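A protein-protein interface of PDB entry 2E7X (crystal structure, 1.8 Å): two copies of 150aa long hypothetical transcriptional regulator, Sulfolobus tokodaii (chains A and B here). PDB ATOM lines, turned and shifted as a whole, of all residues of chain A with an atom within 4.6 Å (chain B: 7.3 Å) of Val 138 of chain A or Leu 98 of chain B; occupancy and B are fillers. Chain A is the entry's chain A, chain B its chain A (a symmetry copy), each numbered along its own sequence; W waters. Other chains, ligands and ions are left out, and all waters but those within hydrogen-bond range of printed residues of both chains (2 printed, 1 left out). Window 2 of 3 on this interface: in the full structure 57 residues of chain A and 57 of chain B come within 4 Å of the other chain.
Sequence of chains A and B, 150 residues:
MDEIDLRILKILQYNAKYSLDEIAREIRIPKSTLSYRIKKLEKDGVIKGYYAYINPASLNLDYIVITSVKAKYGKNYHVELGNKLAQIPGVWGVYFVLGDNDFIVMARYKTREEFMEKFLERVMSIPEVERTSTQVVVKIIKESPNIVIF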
ATOM      1  N   GLN A 135     -11.549 -27.833  33.875  1.00  0.00           N
ATOM      2  CA  GLN A 135     -11.908 -27.324  32.560  1.00  0.00           C
ATOM      3  C   GLN A 135     -11.887 -28.514  31.603  1.00  0.00           C
ATOM      4  O   GLN A 135     -10.847 -29.133  31.395  1.00  0.00           O
ATOM      5  CB  GLN A 135     -10.901 -26.263  32.102  1.00  0.00           C
ATOM      6  CG  GLN A 135     -11.012 -24.932  32.838  1.00  0.00           C
ATOM      7  CD  GLN A 135      -9.869 -23.980  32.506  1.00  0.00           C
ATOM      8  OE1 GLN A 135      -8.731 -24.187  32.925  1.00  0.00           O
ATOM      9  NE2 GLN A 135     -10.169 -22.938  31.746  1.00  0.00           N
ATOM     10  N   VAL A 136     -13.041 -28.843  31.038  1.00  0.00           N
ATOM     11  CA  VAL A 136     -13.122 -29.955  30.101  1.00  0.00           C
ATOM     12  C   VAL A 136     -12.640 -29.521  28.717  1.00  0.00           C
ATOM     13  O   VAL A 136     -13.042 -28.476  28.208  1.00  0.00           O
ATOM     14  CB  VAL A 136     -14.571 -30.496  30.010  1.00  0.00           C
ATOM     15  CG1 VAL A 136     -14.677 -31.553  28.922  1.00  0.00           C
ATOM     16  CG2 VAL A 136     -14.974 -31.082  31.351  1.00  0.00           C
ATOM     17  N   VAL A 137     -11.763 -30.322  28.123  1.00  0.00           N
ATOM     18  CA  VAL A 137     -11.239 -30.025  26.797  1.00  0.00           C
ATOM     19  C   VAL A 137     -12.220 -30.543  25.744  1.00  0.00           C
ATOM     20  O   VAL A 137     -12.434 -31.752  25.621  1.00  0.00           O
ATOM     21  CB  VAL A 137      -9.856 -30.685  26.579  1.00  0.00           C
ATOM     22  CG1 VAL A 137      -9.397 -30.474  25.137  1.00  0.00           C
ATOM     23  CG2 VAL A 137      -8.825 -30.087  27.543  1.00  0.00           C
ATOM     24  N   VAL A 138     -12.815 -29.618  24.997  1.00  0.00           N
ATOM     25  CA  VAL A 138     -13.775 -29.956  23.945  1.00  0.00           C
ATOM     26  C   VAL A 138     -13.027 -30.382  22.688  1.00  0.00           C
ATOM     27  O   VAL A 138     -13.456 -31.279  21.958  1.00  0.00           O
ATOM     28  CB  VAL A 138     -14.654 -28.739  23.579  1.00  0.00           C
ATOM     29  CG1 VAL A 138     -15.675 -29.131  22.514  1.00  0.00           C
ATOM     30  CG2 VAL A 138     -15.348 -28.210  24.816  1.00  0.00           C
ATOM     31  N   LYS A 139     -11.906 -29.722  22.432  1.00  0.00           N
ATOM     32  CA  LYS A 139     -11.114 -30.032  21.258  1.00  0.00           C
ATOM     33  C   LYS A 139      -9.638 -29.735  21.478  1.00  0.00           C
ATOM     34  O   LYS A 139      -9.268 -28.671  21.977  1.00  0.00           O
ATOM     35  CB  LYS A 139     -11.629 -29.227  20.063  1.00  0.00           C
ATOM     36  CG  LYS A 139     -10.962 -29.564  18.738  1.00  0.00           C
ATOM     37  CD  LYS A 139     -11.530 -28.703  17.612  1.00  0.00           C
ATOM     38  CE  LYS A 139     -10.822 -28.954  16.284  1.00  0.00           C
ATOM     39  NZ  LYS A 139     -10.980 -30.354  15.797  1.00  0.00           N
ATOM     40  N   ILE A 140      -8.795 -30.697  21.126  1.00  0.00           N
ATOM     41  CA  ILE A 140      -7.359 -30.506  21.243  1.00  0.00           C
ATOM     42  C   ILE A 140      -6.928 -29.933  19.902  1.00  0.00           C
ATOM     43  O   ILE A 140      -6.970 -30.625  18.885  1.00  0.00           O
ATOM     44  CB  ILE A 140      -6.614 -31.836  21.485  1.00  0.00           C
ATOM     45  CG1 ILE A 140      -6.991 -32.404  22.855  1.00  0.00           C
ATOM     46  CG2 ILE A 140      -5.106 -31.608  21.390  1.00  0.00           C
ATOM     47  CD1 ILE A 140      -6.316 -33.731  23.183  1.00  0.00           C
ATOM     48  N   HIS B  78     -13.373 -20.696  17.498  1.00  0.00           N
ATOM     49  CA  HIS B  78     -12.562 -21.734  18.120  1.00  0.00           C
ATOM     50  C   HIS B  78     -11.515 -22.320  17.178  1.00  0.00           C
ATOM     51  O   HIS B  78     -10.388 -22.598  17.590  1.00  0.00           O
ATOM     52  CB  HIS B  78     -13.454 -22.840  18.705  1.00  0.00           C
ATOM     53  CG  HIS B  78     -14.289 -23.557  17.691  1.00  0.00           C
ATOM     54  ND1 HIS B  78     -14.960 -22.906  16.681  1.00  0.00           N
ATOM     55  CD2 HIS B  78     -14.600 -24.871  17.564  1.00  0.00           C
ATOM     56  CE1 HIS B  78     -15.648 -23.784  15.973  1.00  0.00           C
ATOM     57  NE2 HIS B  78     -15.447 -24.983  16.489  1.00  0.00           N
ATOM     58  N   TYR B  95      -5.653 -25.920  23.705  1.00  0.00           N
ATOM     59  CA  TYR B  95      -6.873 -26.643  24.031  1.00  0.00           C
ATOM     60  C   TYR B  95      -8.110 -25.749  24.060  1.00  0.00           C
ATOM     61  O   TYR B  95      -8.105 -24.710  24.715  1.00  0.00           O
ATOM     62  CB  TYR B  95      -6.714 -27.296  25.411  1.00  0.00           C
ATOM     63  CG  TYR B  95      -5.503 -28.194  25.546  1.00  0.00           C
ATOM     64  CD1 TYR B  95      -5.558 -29.536  25.171  1.00  0.00           C
ATOM     65  CD2 TYR B  95      -4.301 -27.701  26.057  1.00  0.00           C
ATOM     66  CE1 TYR B  95      -4.445 -30.372  25.306  1.00  0.00           C
ATOM     67  CE2 TYR B  95      -3.182 -28.523  26.191  1.00  0.00           C
ATOM     68  CZ  TYR B  95      -3.261 -29.854  25.818  1.00  0.00           C
ATOM     69  OH  TYR B  95      -2.162 -30.666  25.959  1.00  0.00           O
ATOM     70  N   PHE B  96      -9.160 -26.159  23.351  1.00  0.00           N
ATOM     71  CA  PHE B  96     -10.425 -25.421  23.345  1.00  0.00           C
ATOM     72  C   PHE B  96     -11.162 -25.984  24.565  1.00  0.00           C
ATOM     73  O   PHE B  96     -11.452 -27.181  24.620  1.00  0.00           O
ATOM     74  CB  PHE B  96     -11.195 -25.706  22.051  1.00  0.00           C
ATOM     75  CG  PHE B  96     -12.533 -25.027  21.973  1.00  0.00           C
ATOM     76  CD1 PHE B  96     -12.680 -23.692  22.348  1.00  0.00           C
ATOM     77  CD2 PHE B  96     -13.650 -25.721  21.518  1.00  0.00           C
ATOM     78  CE1 PHE B  96     -13.922 -23.058  22.270  1.00  0.00           C
ATOM     79  CE2 PHE B  96     -14.899 -25.096  21.434  1.00  0.00           C
ATOM     80  CZ  PHE B  96     -15.035 -23.765  21.811  1.00  0.00           C
ATOM     81  N   VAL B  97     -11.465 -25.128  25.540  1.00  0.00           N
ATOM     82  CA  VAL B  97     -12.079 -25.602  26.775  1.00  0.00           C
ATOM     83  C   VAL B  97     -13.395 -24.988  27.236  1.00  0.00           C
ATOM     84  O   VAL B  97     -13.817 -23.928  26.767  1.00  0.00           O
ATOM     85  CB  VAL B  97     -11.086 -25.446  27.953  1.00  0.00           C
ATOM     86  CG1 VAL B  97      -9.810 -26.241  27.678  1.00  0.00           C
ATOM     87  CG2 VAL B  97     -10.750 -23.973  28.152  1.00  0.00           C
ATOM     88  N   LEU B  98     -14.020 -25.678  28.187  1.00  0.00           N
ATOM     89  CA  LEU B  98     -15.266 -25.235  28.804  1.00  0.00           C
ATOM     90  C   LEU B  98     -14.893 -24.563  30.124  1.00  0.00           C
ATOM     91  O   LEU B  98     -14.035 -25.058  30.856  1.00  0.00           O
ATOM     92  CB  LEU B  98     -16.177 -26.431  29.079  1.00  0.00           C
ATOM     93  CG  LEU B  98     -16.548 -27.243  27.841  1.00  0.00           C
ATOM     94  CD1 LEU B  98     -17.467 -28.390  28.229  1.00  0.00           C
ATOM     95  CD2 LEU B  98     -17.231 -26.321  26.829  1.00  0.00           C
ATOM     96  N   GLY B  99     -15.537 -23.440  30.423  1.00  0.00           N
ATOM     97  CA  GLY B  99     -15.243 -22.715  31.644  1.00  0.00           C
ATOM     98  C   GLY B  99     -15.180 -21.222  31.374  1.00  0.00           C
ATOM     99  O   GLY B  99     -15.603 -20.771  30.307  1.00  0.00           O
ATOM    100  N   ASP B 100     -14.646 -20.456  32.327  1.00  0.00           N
ATOM    101  CA  ASP B 100     -14.547 -19.003  32.192  1.00  0.00           C
ATOM    102  C   ASP B 100     -13.555 -18.546  31.133  1.00  0.00           C
ATOM    103  O   ASP B 100     -13.467 -17.357  30.835  1.00  0.00           O
ATOM    104  CB  ASP B 100     -14.174 -18.358  33.532  1.00  0.00           C
ATOM    105  CG  ASP B 100     -15.290 -18.443  34.552  1.00  0.00           C
ATOM    106  OD1 ASP B 100     -16.413 -18.844  34.182  1.00  0.00           O
ATOM    107  OD2 ASP B 100     -15.045 -18.101  35.730  1.00  0.00           O
ATOM    108  N   ASN B 101     -12.790 -19.488  30.587  1.00  0.00           N
ATOM    109  CA  ASN B 101     -11.830 -19.180  29.535  1.00  0.00           C
ATOM    110  C   ASN B 101     -12.167 -20.072  28.347  1.00  0.00           C
ATOM    111  O   ASN B 101     -12.885 -21.055  28.500  1.00  0.00           O
ATOM    112  CB  ASN B 101     -10.408 -19.430  30.038  1.00  0.00           C
ATOM    113  CG  ASN B 101     -10.028 -18.488  31.158  1.00  0.00           C
ATOM    114  OD1 ASN B 101      -9.969 -17.274  30.966  1.00  0.00           O
ATOM    115  ND2 ASN B 101      -9.785 -19.038  32.337  1.00  0.00           N
ATOM    116  N   ASP B 102     -11.663 -19.732  27.166  1.00  0.00           N
ATOM    117  CA  ASP B 102     -11.976 -20.515  25.981  1.00  0.00           C
ATOM    118  C   ASP B 102     -10.833 -21.389  25.468  1.00  0.00           C
ATOM    119  O   ASP B 102     -11.074 -22.417  24.840  1.00  0.00           O
ATOM    120  CB  ASP B 102     -12.482 -19.574  24.893  1.00  0.00           C
ATOM    121  CG  ASP B 102     -13.577 -18.655  25.405  1.00  0.00           C
ATOM    122  OD1 ASP B 102     -14.616 -19.168  25.887  1.00  0.00           O
ATOM    123  OD2 ASP B 102     -13.396 -17.422  25.340  1.00  0.00           O
ATOM    124  N   PHE B 103      -9.597 -20.980  25.736  1.00  0.00           N
ATOM    125  CA  PHE B 103      -8.431 -21.763  25.327  1.00  0.00           C
ATOM    126  C   PHE B 103      -7.403 -21.800  26.441  1.00  0.00           C
ATOM    127  O   PHE B 103      -7.291 -20.856  27.222  1.00  0.00           O
ATOM    128  CB  PHE B 103      -7.733 -21.146  24.113  1.00  0.00           C
ATOM    129  CG  PHE B 103      -8.495 -21.272  22.834  1.00  0.00           C
ATOM    130  CD1 PHE B 103      -8.435 -22.441  22.088  1.00  0.00           C
ATOM    131  CD2 PHE B 103      -9.262 -20.211  22.366  1.00  0.00           C
ATOM    132  CE1 PHE B 103      -9.124 -22.550  20.887  1.00  0.00           C
ATOM    133  CE2 PHE B 103      -9.954 -20.316  21.165  1.00  0.00           C
ATOM    134  CZ  PHE B 103      -9.885 -21.486  20.430  1.00  0.00           C
HETATM  135  O   HOH W   1     -15.217 -27.842  32.569  1.00  0.00           O
HETATM  136  O   HOH W   2      -7.616 -21.231  33.432  1.00  0.00           O
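Val 97 of chain B touches Gln 135 of chain A. Leu 98 of chain B touches Gln 135 of chain A. Gln 135 of chain A touches Asn 101 of chain B (NE2 to CB, 3.9 Å). Val 136 of chain A touches Val 97 of chain B. Val 137 of chain A touches Tyr 95 of chain B (CG1 to CD1, 3.95 Å). Val 137 of chain A touches Phe 96 of chain B (CA to O, 3.6 Å). CG2 of Val 137 of chain A touches CG1 of Val 97 of chain B, 3.97 Å away. Leu 98 of chain B touches Val 138 of chain A. Lys 139 of chain A touches Tyr 95 of chain B (O to CA, 3.8 Å). Ile 140 of chain A touches Tyr 95 of chain B.
Water W1 lies within hydrogen-bond range of the backbone NH of Val 136 of chain A (2.8 Å) and the backbone carbonyl oxygen of Leu 98 of chain B (3.5 Å). Water W2 lies within hydrogen-bond range of OE1 of Gln 135 of chain A (3.2 Å) and ND2 of Asn 101 of chain B (3.3 Å).
Val 138 of chain A touches two residues of chain B. Leu 98 of chain B touches just these residues of chain A: Gln 135 (3.5 Å), Val 136 (3.0 Å) and Val 138 (3.3 Å). Printed residues of chain B within 4 Å of Val 136 of chain A: Val 97 (3.4 Å) and Leu 98 (3.0 Å). Printed residues of chain B within 4 Å of Gln 135 of chain A: Val 97 (3.8 Å), Leu 98 (3.5 Å) and Asn 101 (3.9 Å). Printed residues of chain B within 4 Å of Ile 140 of chain A: Tyr 95 (3.96 Å). The nearest residue of chain B that does not touch Val 138 of chain A is Val 97 of chain B (4.5 Å). The nearest printed residue of chain A that does not touch Leu 98 of chain B is Val 137 of chain A (5.2 Å). The nearest printed residue of chain B that does not touch Gln 135 of chain A is Gly 99 of chain B (4.9 Å).
The backbone NH (N) of Val 97 of chain B sits at hydrogen-bond distance from the backbone carbonyl oxygen (O) of Asp 102 of chain B, 2.8 Å away.
Hydrophobic or aromatic side chains of chain B within 4 Å of the printed part of chain A: Tyr 95, Phe 96, Val 97 and Leu 98. Hydrophobic or aromatic side chains of chain A that line the printed part of chain B: Val 136, Val 137, Val 138 and Ile 140. Among the printed residues, no Asp or Glu carboxylate lies within 4 Å of a Lys or Arg side-chain nitrogen of the other chain.
The backbone NH (N) of Leu 98 of chain B sits at hydrogen-bond distance from the backbone carbonyl oxygen (O) of Val 136 of chain A, 3.0 Å away. The backbone NH of Val 138 of chain A lies within hydrogen-bond range of the backbone carbonyl oxygen of Phe 96 of chain B (2.8 Å). O of Lys 139 of chain A is in hydrogen-bond range of N of Phe 96 of chain B (2.9 Å).
No position is printed for both chains. Of the 13 pairs that touch across the chains among the printed residues, none has its exchanged pair printed and touching as well.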
